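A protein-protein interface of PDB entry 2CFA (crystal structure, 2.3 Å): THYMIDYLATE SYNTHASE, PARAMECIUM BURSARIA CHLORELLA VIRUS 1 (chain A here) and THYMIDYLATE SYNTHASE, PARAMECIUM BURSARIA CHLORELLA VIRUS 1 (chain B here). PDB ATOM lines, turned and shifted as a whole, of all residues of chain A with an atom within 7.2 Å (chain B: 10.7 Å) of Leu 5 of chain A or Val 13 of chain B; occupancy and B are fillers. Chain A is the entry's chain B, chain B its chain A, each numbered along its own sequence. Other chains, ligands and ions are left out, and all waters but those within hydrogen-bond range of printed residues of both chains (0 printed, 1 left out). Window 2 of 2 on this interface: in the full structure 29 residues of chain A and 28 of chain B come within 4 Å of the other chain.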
ATOM      1  N   ALA A   3      -9.069  -5.731   6.411  1.00  0.00           N
ATOM      2  CA  ALA A   3      -8.729  -7.098   6.021  1.00  0.00           C
ATOM      3  C   ALA A   3      -8.074  -7.872   7.164  1.00  0.00           C
ATOM      4  O   ALA A   3      -7.342  -7.304   7.970  1.00  0.00           O
ATOM      5  CB  ALA A   3      -7.809  -7.081   4.804  1.00  0.00           C
ATOM      6  N   LYS A   4      -8.333  -9.172   7.233  1.00  0.00           N
ATOM      7  CA  LYS A   4      -7.570 -10.033   8.140  1.00  0.00           C
ATOM      8  C   LYS A   4      -7.136 -11.331   7.480  1.00  0.00           C
ATOM      9  O   LYS A   4      -7.795 -11.817   6.557  1.00  0.00           O
ATOM     10  CB  LYS A   4      -8.316 -10.310   9.454  1.00  0.00           C
ATOM     11  CG  LYS A   4      -9.713 -10.895   9.296  1.00  0.00           C
ATOM     12  CD  LYS A   4     -10.029 -11.949  10.366  1.00  0.00           C
ATOM     13  CE  LYS A   4      -9.982 -11.407  11.789  1.00  0.00           C
ATOM     14  NZ  LYS A   4      -9.992 -12.549  12.777  1.00  0.00           N
ATOM     15  N   LEU A   5      -6.018 -11.879   7.945  1.00  0.00           N
ATOM     16  CA  LEU A   5      -5.565 -13.178   7.476  1.00  0.00           C
ATOM     17  C   LEU A   5      -6.499 -14.243   8.041  1.00  0.00           C
ATOM     18  O   LEU A   5      -6.855 -14.206   9.221  1.00  0.00           O
ATOM     19  CB  LEU A   5      -4.113 -13.431   7.888  1.00  0.00           C
ATOM     20  CG  LEU A   5      -3.403 -14.720   7.461  1.00  0.00           C
ATOM     21  CD1 LEU A   5      -3.329 -14.870   5.936  1.00  0.00           C
ATOM     22  CD2 LEU A   5      -2.026 -14.737   8.061  1.00  0.00           C
ATOM     23  N   ILE A   6      -6.926 -15.167   7.182  1.00  0.00           N
ATOM     24  CA  ILE A   6      -7.815 -16.242   7.585  1.00  0.00           C
ATOM     25  C   ILE A   6      -7.025 -17.542   7.521  1.00  0.00           C
ATOM     26  O   ILE A   6      -7.179 -18.418   8.366  1.00  0.00           O
ATOM     27  CB  ILE A   6      -9.078 -16.278   6.674  1.00  0.00           C
ATOM     28  CG1 ILE A   6     -10.011 -15.093   6.983  1.00  0.00           C
ATOM     29  CG2 ILE A   6      -9.817 -17.633   6.731  1.00  0.00           C
ATOM     30  CD1 ILE A   6     -10.591 -15.032   8.409  1.00  0.00           C
ATOM     31  N   SER A   7      -6.138 -17.634   6.532  1.00  0.00           N
ATOM     32  CA  SER A   7      -5.545 -18.902   6.165  1.00  0.00           C
ATOM     33  C   SER A   7      -4.420 -18.715   5.176  1.00  0.00           C
ATOM     34  O   SER A   7      -4.492 -17.872   4.283  1.00  0.00           O
ATOM     35  CB  SER A   7      -6.614 -19.785   5.510  1.00  0.00           C
ATOM     36  OG  SER A   7      -6.023 -20.941   4.950  1.00  0.00           O
ATOM     37  N   VAL A   8      -3.399 -19.547   5.308  1.00  0.00           N
ATOM     38  CA  VAL A   8      -2.299 -19.552   4.365  1.00  0.00           C
ATOM     39  C   VAL A   8      -1.649 -20.935   4.295  1.00  0.00           C
ATOM     40  O   VAL A   8      -1.689 -21.720   5.249  1.00  0.00           O
ATOM     41  CB  VAL A   8      -1.251 -18.407   4.698  1.00  0.00           C
ATOM     42  CG1 VAL A   8      -0.604 -18.621   6.088  1.00  0.00           C
ATOM     43  CG2 VAL A   8      -0.196 -18.251   3.592  1.00  0.00           C
ATOM     44  N   PHE A  61      -0.843 -20.039  -1.296  1.00  0.00           N
ATOM     45  CA  PHE A  61      -2.233 -19.643  -1.386  1.00  0.00           C
ATOM     46  C   PHE A  61      -2.488 -19.027  -0.047  1.00  0.00           C
ATOM     47  O   PHE A  61      -2.017 -19.540   0.985  1.00  0.00           O
ATOM     48  CB  PHE A  61      -3.077 -20.893  -1.508  1.00  0.00           C
ATOM     49  CG  PHE A  61      -4.469 -20.681  -2.001  1.00  0.00           C
ATOM     50  CD1 PHE A  61      -5.546 -20.780  -1.129  1.00  0.00           C
ATOM     51  CD2 PHE A  61      -4.725 -20.488  -3.352  1.00  0.00           C
ATOM     52  CE1 PHE A  61      -6.844 -20.658  -1.587  1.00  0.00           C
ATOM     53  CE2 PHE A  61      -6.039 -20.358  -3.826  1.00  0.00           C
ATOM     54  CZ  PHE A  61      -7.092 -20.454  -2.952  1.00  0.00           C
ATOM     55  N   MET A  62      -3.244 -17.937  -0.077  1.00  0.00           N
ATOM     56  CA  MET A  62      -3.559 -17.164   1.096  1.00  0.00           C
ATOM     57  C   MET A  62      -5.001 -16.751   0.966  1.00  0.00           C
ATOM     58  O   MET A  62      -5.486 -16.540  -0.137  1.00  0.00           O
ATOM     59  CB  MET A  62      -2.656 -15.923   1.147  1.00  0.00           C
ATOM     60  CG  MET A  62      -2.899 -14.997   2.327  1.00  0.00           C
ATOM     61  SD  MET A  62      -1.606 -13.751   2.536  1.00  0.00           S
ATOM     62  CE  MET A  62      -1.971 -12.681   1.127  1.00  0.00           C
ATOM     63  N   THR A  63      -5.698 -16.645   2.091  1.00  0.00           N
ATOM     64  CA  THR A  63      -7.046 -16.097   2.070  1.00  0.00           C
ATOM     65  C   THR A  63      -7.293 -15.031   3.114  1.00  0.00           C
ATOM     66  O   THR A  63      -6.821 -15.124   4.255  1.00  0.00           O
ATOM     67  CB  THR A  63      -8.206 -17.195   1.957  1.00  0.00           C
ATOM     68  OG1 THR A  63      -9.263 -16.944   2.894  1.00  0.00           O
ATOM     69  CG2 THR A  63      -7.705 -18.590   2.110  1.00  0.00           C
ATOM     70  N   LEU A  64      -7.987 -13.983   2.690  1.00  0.00           N
ATOM     71  CA  LEU A  64      -8.253 -12.852   3.546  1.00  0.00           C
ATOM     72  C   LEU A  64      -9.725 -12.591   3.614  1.00  0.00           C
ATOM     73  O   LEU A  64     -10.454 -12.782   2.637  1.00  0.00           O
ATOM     74  CB  LEU A  64      -7.530 -11.572   3.068  1.00  0.00           C
ATOM     75  CG  LEU A  64      -6.013 -11.553   2.835  1.00  0.00           C
ATOM     76  CD1 LEU A  64      -5.487 -10.129   2.642  1.00  0.00           C
ATOM     77  CD2 LEU A  64      -5.274 -12.222   3.939  1.00  0.00           C
ATOM     78  N   GLU A  65     -10.150 -12.150   4.789  1.00  0.00           N
ATOM     79  CA  GLU A  65     -11.494 -11.658   4.992  1.00  0.00           C
ATOM     80  C   GLU A  65     -11.470 -10.155   4.780  1.00  0.00           C
ATOM     81  O   GLU A  65     -10.672  -9.443   5.389  1.00  0.00           O
ATOM     82  CB  GLU A  65     -11.950 -11.988   6.403  1.00  0.00           C
ATOM     83  CG  GLU A  65     -13.329 -11.492   6.754  1.00  0.00           C
ATOM     84  CD  GLU A  65     -13.583 -11.573   8.238  1.00  0.00           C
ATOM     85  OE1 GLU A  65     -14.397 -12.412   8.655  1.00  0.00           O
ATOM     86  OE2 GLU A  65     -12.942 -10.813   8.993  1.00  0.00           O
ATOM     87  N   TYR A 167     -14.655 -13.566   1.807  1.00  0.00           N
ATOM     88  CA  TYR A 167     -13.328 -14.171   1.768  1.00  0.00           C
ATOM     89  C   TYR A 167     -12.797 -13.970   0.371  1.00  0.00           C
ATOM     90  O   TYR A 167     -13.543 -14.063  -0.607  1.00  0.00           O
ATOM     91  CB  TYR A 167     -13.384 -15.671   2.056  1.00  0.00           C
ATOM     92  CG  TYR A 167     -13.507 -16.072   3.512  1.00  0.00           C
ATOM     93  CD1 TYR A 167     -13.756 -15.131   4.520  1.00  0.00           C
ATOM     94  CD2 TYR A 167     -13.410 -17.414   3.873  1.00  0.00           C
ATOM     95  CE1 TYR A 167     -13.874 -15.526   5.853  1.00  0.00           C
ATOM     96  CE2 TYR A 167     -13.532 -17.823   5.192  1.00  0.00           C
ATOM     97  CZ  TYR A 167     -13.763 -16.882   6.179  1.00  0.00           C
ATOM     98  OH  TYR A 167     -13.874 -17.314   7.485  1.00  0.00           O
ATOM     99  N   ILE A 201      -0.876  -7.105   5.366  1.00  0.00           N
ATOM    100  CA  ILE A 201      -0.911  -8.532   5.690  1.00  0.00           C
ATOM    101  C   ILE A 201       0.072  -9.331   4.825  1.00  0.00           C
ATOM    102  O   ILE A 201       0.822 -10.174   5.330  1.00  0.00           O
ATOM    103  CB  ILE A 201      -2.365  -9.069   5.580  1.00  0.00           C
ATOM    104  CG1 ILE A 201      -3.227  -8.423   6.669  1.00  0.00           C
ATOM    105  CG2 ILE A 201      -2.418 -10.605   5.677  1.00  0.00           C
ATOM    106  CD1 ILE A 201      -4.668  -8.353   6.334  1.00  0.00           C
ATOM    107  N   PHE A 202       0.088  -9.036   3.529  1.00  0.00           N
ATOM    108  CA  PHE A 202       1.033  -9.647   2.596  1.00  0.00           C
ATOM    109  C   PHE A 202       2.491  -9.424   3.016  1.00  0.00           C
ATOM    110  O   PHE A 202       3.269 -10.387   3.118  1.00  0.00           O
ATOM    111  CB  PHE A 202       0.779  -9.108   1.181  1.00  0.00           C
ATOM    112  CG  PHE A 202       1.578  -9.797   0.105  1.00  0.00           C
ATOM    113  CD1 PHE A 202       0.949 -10.647  -0.803  1.00  0.00           C
ATOM    114  CD2 PHE A 202       2.954  -9.592  -0.007  1.00  0.00           C
ATOM    115  CE1 PHE A 202       1.677 -11.277  -1.807  1.00  0.00           C
ATOM    116  CE2 PHE A 202       3.689 -10.215  -0.998  1.00  0.00           C
ATOM    117  CZ  PHE A 202       3.052 -11.060  -1.903  1.00  0.00           C
ATOM    118  N   LYS A 204       3.626  -8.703   5.958  1.00  0.00           N
ATOM    119  CA  LYS A 204       3.865  -9.511   7.158  1.00  0.00           C
ATOM    120  C   LYS A 204       4.162 -10.987   6.838  1.00  0.00           C
ATOM    121  O   LYS A 204       5.111 -11.550   7.378  1.00  0.00           O
ATOM    122  CB  LYS A 204       2.669  -9.411   8.095  1.00  0.00           C
ATOM    123  CG  LYS A 204       2.994  -9.395   9.584  1.00  0.00           C
ATOM    124  CD  LYS A 204       1.953  -8.552  10.341  1.00  0.00           C
ATOM    125  CE  LYS A 204       2.137  -7.053  10.056  1.00  0.00           C
ATOM    126  NZ  LYS A 204       1.078  -6.186  10.670  1.00  0.00           N
ATOM    127  N   GLU A 205       3.365 -11.610   5.961  1.00  0.00           N
ATOM    128  CA  GLU A 205       3.532 -13.045   5.667  1.00  0.00           C
ATOM    129  C   GLU A 205       4.693 -13.326   4.733  1.00  0.00           C
ATOM    130  O   GLU A 205       5.333 -14.383   4.819  1.00  0.00           O
ATOM    131  CB  GLU A 205       2.262 -13.667   5.064  1.00  0.00           C
ATOM    132  CG  GLU A 205       1.119 -13.841   6.029  1.00  0.00           C
ATOM    133  CD  GLU A 205       1.536 -14.563   7.297  1.00  0.00           C
ATOM    134  OE1 GLU A 205       1.975 -15.735   7.191  1.00  0.00           O
ATOM    135  OE2 GLU A 205       1.436 -13.933   8.384  1.00  0.00           O
ATOM    136  N   PHE A 206       4.945 -12.390   3.831  1.00  0.00           N
ATOM    137  CA  PHE A 206       5.970 -12.564   2.802  1.00  0.00           C
ATOM    138  C   PHE A 206       6.964 -11.391   2.803  1.00  0.00           C
ATOM    139  O   PHE A 206       7.076 -10.686   1.796  1.00  0.00           O
ATOM    140  CB  PHE A 206       5.295 -12.757   1.417  1.00  0.00           C
ATOM    141  CG  PHE A 206       4.334 -13.923   1.377  1.00  0.00           C
ATOM    142  CD1 PHE A 206       2.980 -13.732   1.622  1.00  0.00           C
ATOM    143  CD2 PHE A 206       4.798 -15.215   1.147  1.00  0.00           C
ATOM    144  CE1 PHE A 206       2.100 -14.803   1.622  1.00  0.00           C
ATOM    145  CE2 PHE A 206       3.923 -16.299   1.141  1.00  0.00           C
ATOM    146  CZ  PHE A 206       2.571 -16.097   1.378  1.00  0.00           C
ATOM    147  N   THR B   9      -3.036 -25.709   2.906  1.00  0.00           N
ATOM    148  CA  THR B   9      -3.734 -24.657   3.657  1.00  0.00           C
ATOM    149  C   THR B   9      -3.887 -24.904   5.173  1.00  0.00           C
ATOM    150  O   THR B   9      -4.469 -25.901   5.608  1.00  0.00           O
ATOM    151  CB  THR B   9      -5.143 -24.455   3.000  1.00  0.00           C
ATOM    152  OG1 THR B   9      -4.981 -23.673   1.818  1.00  0.00           O
ATOM    153  CG2 THR B   9      -6.155 -23.756   3.922  1.00  0.00           C
ATOM    154  N   LYS B  10      -3.385 -23.978   5.978  1.00  0.00           N
ATOM    155  CA  LYS B  10      -3.681 -23.996   7.416  1.00  0.00           C
ATOM    156  C   LYS B  10      -4.287 -22.675   7.904  1.00  0.00           C
ATOM    157  O   LYS B  10      -3.644 -21.634   7.815  1.00  0.00           O
ATOM    158  CB  LYS B  10      -2.437 -24.353   8.239  1.00  0.00           C
ATOM    159  CG  LYS B  10      -2.751 -24.517   9.741  1.00  0.00           C
ATOM    160  CD  LYS B  10      -1.548 -24.933  10.546  1.00  0.00           C
ATOM    161  CE  LYS B  10      -1.783 -24.714  12.049  1.00  0.00           C
ATOM    162  NZ  LYS B  10      -2.921 -25.543  12.571  1.00  0.00           N
ATOM    163  N   PRO B  11      -5.522 -22.714   8.441  1.00  0.00           N
ATOM    164  CA  PRO B  11      -6.196 -21.516   8.968  1.00  0.00           C
ATOM    165  C   PRO B  11      -5.457 -20.935  10.178  1.00  0.00           C
ATOM    166  O   PRO B  11      -4.858 -21.687  10.939  1.00  0.00           O
ATOM    167  CB  PRO B  11      -7.561 -22.048   9.416  1.00  0.00           C
ATOM    168  CG  PRO B  11      -7.718 -23.330   8.716  1.00  0.00           C
ATOM    169  CD  PRO B  11      -6.360 -23.911   8.608  1.00  0.00           C
ATOM    170  N   VAL B  12      -5.487 -19.615  10.331  1.00  0.00           N
ATOM    171  CA  VAL B  12      -4.770 -18.943  11.428  1.00  0.00           C
ATOM    172  C   VAL B  12      -5.739 -18.405  12.473  1.00  0.00           C
ATOM    173  O   VAL B  12      -5.324 -17.770  13.440  1.00  0.00           O
ATOM    174  CB  VAL B  12      -3.853 -17.776  10.939  1.00  0.00           C
ATOM    175  CG1 VAL B  12      -2.847 -18.262   9.908  1.00  0.00           C
ATOM    176  CG2 VAL B  12      -4.676 -16.615  10.404  1.00  0.00           C
ATOM    177  N   VAL B  13      -7.027 -18.666  12.280  1.00  0.00           N
ATOM    178  CA  VAL B  13      -8.041 -18.153  13.190  1.00  0.00           C
ATOM    179  C   VAL B  13      -8.393 -19.139  14.303  1.00  0.00           C
ATOM    180  O   VAL B  13      -8.192 -20.346  14.163  1.00  0.00           O
ATOM    181  CB  VAL B  13      -9.307 -17.695  12.441  1.00  0.00           C
ATOM    182  CG1 VAL B  13      -9.039 -16.351  11.765  1.00  0.00           C
ATOM    183  CG2 VAL B  13      -9.764 -18.745  11.439  1.00  0.00           C
ATOM    184  N   GLU B  14      -8.915 -18.598  15.406  1.00  0.00           N
ATOM    185  CA  GLU B  14      -9.192 -19.360  16.617  1.00  0.00           C
ATOM    186  C   GLU B  14     -10.332 -20.362  16.439  1.00  0.00           C
ATOM    187  O   GLU B  14     -11.431 -20.009  15.985  1.00  0.00           O
ATOM    188  CB  GLU B  14      -9.489 -18.413  17.789  1.00  0.00           C
ATOM    189  CG  GLU B  14      -8.245 -17.782  18.439  1.00  0.00           C
ATOM    190  CD  GLU B  14      -7.551 -18.684  19.472  1.00  0.00           C
ATOM    191  OE1 GLU B  14      -6.621 -18.185  20.155  1.00  0.00           O
ATOM    192  OE2 GLU B  14      -7.924 -19.879  19.613  1.00  0.00           O
ATOM    193  N   GLY B  15     -10.051 -21.614  16.804  1.00  0.00           N
ATOM    194  CA  GLY B  15     -11.046 -22.683  16.782  1.00  0.00           C
ATOM    195  C   GLY B  15     -11.040 -23.500  15.506  1.00  0.00           C
ATOM    196  O   GLY B  15     -11.703 -24.539  15.426  1.00  0.00           O
ATOM    197  N   VAL B  16     -10.289 -23.024  14.511  1.00  0.00           N
ATOM    198  CA  VAL B  16     -10.182 -23.682  13.213  1.00  0.00           C
ATOM    199  C   VAL B  16      -8.709 -23.976  12.933  1.00  0.00           C
ATOM    200  O   VAL B  16      -7.931 -23.068  12.619  1.00  0.00           O
ATOM    201  CB  VAL B  16     -10.799 -22.808  12.091  1.00  0.00           C
ATOM    202  CG1 VAL B  16     -10.856 -23.568  10.803  1.00  0.00           C
ATOM    203  CG2 VAL B  16     -12.200 -22.333  12.483  1.00  0.00           C
ATOM    204  N   ASN B  17      -8.337 -25.246  13.063  1.00  0.00           N
ATOM    205  CA  ASN B  17      -6.934 -25.666  13.034  1.00  0.00           C
ATOM    206  C   ASN B  17      -6.512 -26.425  11.783  1.00  0.00           C
ATOM    207  O   ASN B  17      -5.327 -26.702  11.608  1.00  0.00           O
ATOM    208  CB  ASN B  17      -6.605 -26.547  14.253  1.00  0.00           C
ATOM    209  CG  ASN B  17      -6.897 -25.864  15.574  1.00  0.00           C
ATOM    210  OD1 ASN B  17      -7.459 -26.479  16.487  1.00  0.00           O
ATOM    211  ND2 ASN B  17      -6.516 -24.579  15.688  1.00  0.00           N
ATOM    212  N   THR B  18      -7.472 -26.807  10.944  1.00  0.00           N
ATOM    213  CA  THR B  18      -7.155 -27.527   9.704  1.00  0.00           C
ATOM    214  C   THR B  18      -7.841 -26.901   8.488  1.00  0.00           C
ATOM    215  O   THR B  18      -8.831 -26.198   8.630  1.00  0.00           O
ATOM    216  CB  THR B  18      -7.523 -29.025   9.774  1.00  0.00           C
ATOM    217  OG1 THR B  18      -8.945 -29.182   9.704  1.00  0.00           O
ATOM    218  CG2 THR B  18      -6.992 -29.676  11.049  1.00  0.00           C
ATOM    219  N   ALA B  19      -7.305 -27.157   7.298  1.00  0.00           N
ATOM    220  CA  ALA B  19      -7.981 -26.764   6.047  1.00  0.00           C
ATOM    221  C   ALA B  19      -9.453 -27.211   6.011  1.00  0.00           C
ATOM    222  O   ALA B  19     -10.329 -26.436   5.657  1.00  0.00           O
ATOM    223  CB  ALA B  19      -7.216 -27.313   4.829  1.00  0.00           C
ATOM    224  N   GLU B  21     -11.534 -28.080   8.496  1.00  0.00           N
ATOM    225  CA  GLU B  21     -12.309 -27.409   9.525  1.00  0.00           C
ATOM    226  C   GLU B  21     -12.744 -26.048   9.032  1.00  0.00           C
ATOM    227  O   GLU B  21     -13.821 -25.591   9.369  1.00  0.00           O
ATOM    228  CB  GLU B  21     -11.491 -27.242  10.815  1.00  0.00           C
ATOM    229  CG  GLU B  21     -11.381 -28.499  11.661  1.00  0.00           C
ATOM    230  CD  GLU B  21     -10.666 -28.248  12.979  1.00  0.00           C
ATOM    231  OE1 GLU B  21      -9.849 -29.095  13.372  1.00  0.00           O
ATOM    232  OE2 GLU B  21     -10.916 -27.202  13.619  1.00  0.00           O
ATOM    233  N   LEU B  22     -11.887 -25.394   8.247  1.00  0.00           N
ATOM    234  CA  LEU B  22     -12.233 -24.119   7.626  1.00  0.00           C
ATOM    235  C   LEU B  22     -13.284 -24.321   6.552  1.00  0.00           C
ATOM    236  O   LEU B  22     -14.220 -23.529   6.449  1.00  0.00           O
ATOM    237  CB  LEU B  22     -10.997 -23.402   7.055  1.00  0.00           C
ATOM    238  CG  LEU B  22     -11.244 -22.039   6.372  1.00  0.00           C
ATOM    239  CD1 LEU B  22     -11.909 -21.019   7.318  1.00  0.00           C
ATOM    240  CD2 LEU B  22      -9.966 -21.465   5.763  1.00  0.00           C
ATOM    241  N   ILE B  23     -13.141 -25.372   5.749  1.00  0.00           N
ATOM    242  CA  ILE B  23     -14.192 -25.706   4.767  1.00  0.00           C
ATOM    243  C   ILE B  23     -15.534 -25.938   5.457  1.00  0.00           C
ATOM    244  O   ILE B  23     -16.542 -25.394   5.020  1.00  0.00           O
ATOM    245  CB  ILE B  23     -13.837 -26.924   3.885  1.00  0.00           C
ATOM    246  CG1 ILE B  23     -12.657 -26.590   2.962  1.00  0.00           C
ATOM    247  CG2 ILE B  23     -15.055 -27.369   3.057  1.00  0.00           C
ATOM    248  CD1 ILE B  23     -12.059 -27.785   2.301  1.00  0.00           C
ATOM    249  N   TYR B  25     -16.434 -24.999   8.526  1.00  0.00           N
ATOM    250  CA  TYR B  25     -16.825 -23.745   9.138  1.00  0.00           C
ATOM    251  C   TYR B  25     -17.574 -22.869   8.136  1.00  0.00           C
ATOM    252  O   TYR B  25     -18.598 -22.269   8.475  1.00  0.00           O
ATOM    253  CB  TYR B  25     -15.600 -23.011   9.702  1.00  0.00           C
ATOM    254  CG  TYR B  25     -15.907 -21.627  10.217  1.00  0.00           C
ATOM    255  CD1 TYR B  25     -16.561 -21.442  11.434  1.00  0.00           C
ATOM    256  CD2 TYR B  25     -15.564 -20.501   9.480  1.00  0.00           C
ATOM    257  CE1 TYR B  25     -16.860 -20.164  11.909  1.00  0.00           C
ATOM    258  CE2 TYR B  25     -15.858 -19.223   9.938  1.00  0.00           C
ATOM    259  CZ  TYR B  25     -16.506 -19.061  11.154  1.00  0.00           C
ATOM    260  OH  TYR B  25     -16.793 -17.791  11.615  1.00  0.00           O
ATOM    261  N   ALA B  26     -17.063 -22.811   6.905  1.00  0.00           N
ATOM    262  CA  ALA B  26     -17.685 -22.015   5.847  1.00  0.00           C
ATOM    263  C   ALA B  26     -19.069 -22.555   5.459  1.00  0.00           C
ATOM    264  O   ALA B  26     -19.978 -21.778   5.178  1.00  0.00           O
ATOM    265  CB  ALA B  26     -16.768 -21.930   4.639  1.00  0.00           C
ATOM    266  N   ARG B  28     -21.015 -24.200   7.509  1.00  0.00           N
ATOM    267  CA  ARG B  28     -21.860 -23.977   8.682  1.00  0.00           C
ATOM    268  C   ARG B  28     -22.467 -22.571   8.719  1.00  0.00           C
ATOM    269  O   ARG B  28     -23.680 -22.430   8.836  1.00  0.00           O
ATOM    270  CB  ARG B  28     -21.095 -24.291   9.973  1.00  0.00           C
ATOM    271  CG  ARG B  28     -21.367 -25.690  10.523  1.00  0.00           C
ATOM    272  CD  ARG B  28     -20.101 -26.377  11.002  1.00  0.00           C
ATOM    273  NE  ARG B  28     -19.236 -25.480  11.767  1.00  0.00           N
ATOM    274  CZ  ARG B  28     -17.958 -25.720  12.040  1.00  0.00           C
ATOM    275  NH1 ARG B  28     -17.375 -26.839  11.619  1.00  0.00           N
ATOM    276  NH2 ARG B  28     -17.260 -24.839  12.734  1.00  0.00           N
ATOM    277  N   VAL B  29     -21.638 -21.536   8.607  1.00  0.00           N
ATOM    278  CA  VAL B  29     -22.147 -20.160   8.529  1.00  0.00           C
ATOM    279  C   VAL B  29     -22.832 -19.922   7.169  1.00  0.00           C
ATOM    280  O   VAL B  29     -22.777 -18.834   6.583  1.00  0.00           O
ATOM    281  CB  VAL B  29     -21.046 -19.110   8.891  1.00  0.00           C
ATOM    282  CG1 VAL B  29     -19.782 -19.328   8.086  1.00  0.00           C
ATOM    283  CG2 VAL B  29     -21.562 -17.680   8.743  1.00  0.00           C
ATOM    284  N   THR B  59     -11.470 -22.491  -0.602  1.00  0.00           N
ATOM    285  CA  THR B  59     -10.792 -21.823   0.513  1.00  0.00           C
ATOM    286  C   THR B  59      -9.557 -22.605   0.949  1.00  0.00           C
ATOM    287  O   THR B  59      -8.670 -22.061   1.618  1.00  0.00           O
ATOM    288  CB  THR B  59     -11.733 -21.616   1.751  1.00  0.00           C
ATOM    289  OG1 THR B  59     -12.111 -22.886   2.316  1.00  0.00           O
ATOM    290  CG2 THR B  59     -12.995 -20.863   1.348  1.00  0.00           C
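NZ of Lys 10 of chain B lies within hydrogen-bond range of O of Asn 17 of chain B (2.8 Å).
O of Ser 7 of chain A is in hydrogen-bond range of N of Thr 63 of chain A, at 2.8 Å.
The backbone NH (N) of Ile 6 of chain A lies within hydrogen-bond range of the backbone carbonyl oxygen (O) of Thr 63 of chain A (2.9 Å).
Of the 17 printed residues of chain A, 7 touch a printed residue of chain B.
Along chain A the printed residues that touch a printed residue of chain B span positions 5 to 167.
Hydrophobic or aromatic side chains of chain B within 4 Å of the printed part of chain A: Pro 11, Val 12, Val 13, Leu 22 and Tyr 25.
Among the printed residues, 15 pairs touch across the chains.
Among the printed residues, no Asp or Glu carboxylate lies within 4 Å of a Lys or Arg side-chain nitrogen of the other chain.
Among the printed residues, merely in contact across the chains: Leu 5 of chain A with Val 12 of chain B (3.5 Å), Leu 5 of chain A with Val 13 of chain B (3.98 Å), Ile 6 of chain A with Pro 11 of chain B (3.3 Å), Ile 6 of chain A with Val 13 of chain B (3.9 Å), Ile 6 of chain A with Leu 22 of chain B (3.96 Å), Ser 7 of chain A with Thr 9 of chain B (3.0 Å), Ser 7 of chain A with Lys 10 of chain B (3.7 Å), Ser 7 of chain A with Pro 11 of chain B (3.9 Å), Ser 7 of chain A with Leu 22 of chain B (3.8 Å), Val 8 of chain A with Thr 9 of chain B (3.9 Å), Phe 61 of chain A with Thr 59 of chain B (3.9 Å), Thr 63 of chain A with Thr 59 of chain B (3.6 Å) and Tyr 167 of chain A with Tyr 25 of chain B (3.7 Å).
The backbone NH of Val 12 of chain B lies within hydrogen-bond range of the backbone carbonyl oxygen of Ile 6 of chain A (2.9 Å).
The backbone NH (N) of Lys 10 of chain B is in hydrogen-bond range of the backbone carbonyl oxygen (O) of Val 8 of chain A.
Printed residues of chain B within 4 Å of Leu 5 of chain A: Val 12 and Val 13.
Of the printed residues of chain A, Val 13 of chain B touches Leu 5 (3.98 Å) and Ile 6 (3.9 Å).
Of the printed residues of chain B, Ile 6 of chain A touches Pro 11, Val 12, Val 13 and Leu 22.
Of the printed residues of chain A, Leu 22 of chain B touches Ile 6 (3.96 Å) and Ser 7 (3.8 Å).
Of the printed residues of chain A, Val 12 of chain B touches Leu 5 (3.5 Å) and Ile 6 (2.9 Å).
The nearest printed residue of chain A that does not touch Val 13 of chain B is Lys 4 of chain A (4.05 Å).
The nearest printed residue of chain A that does not touch Pro 11 of chain B is Val 8 of chain A (4.9 Å).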
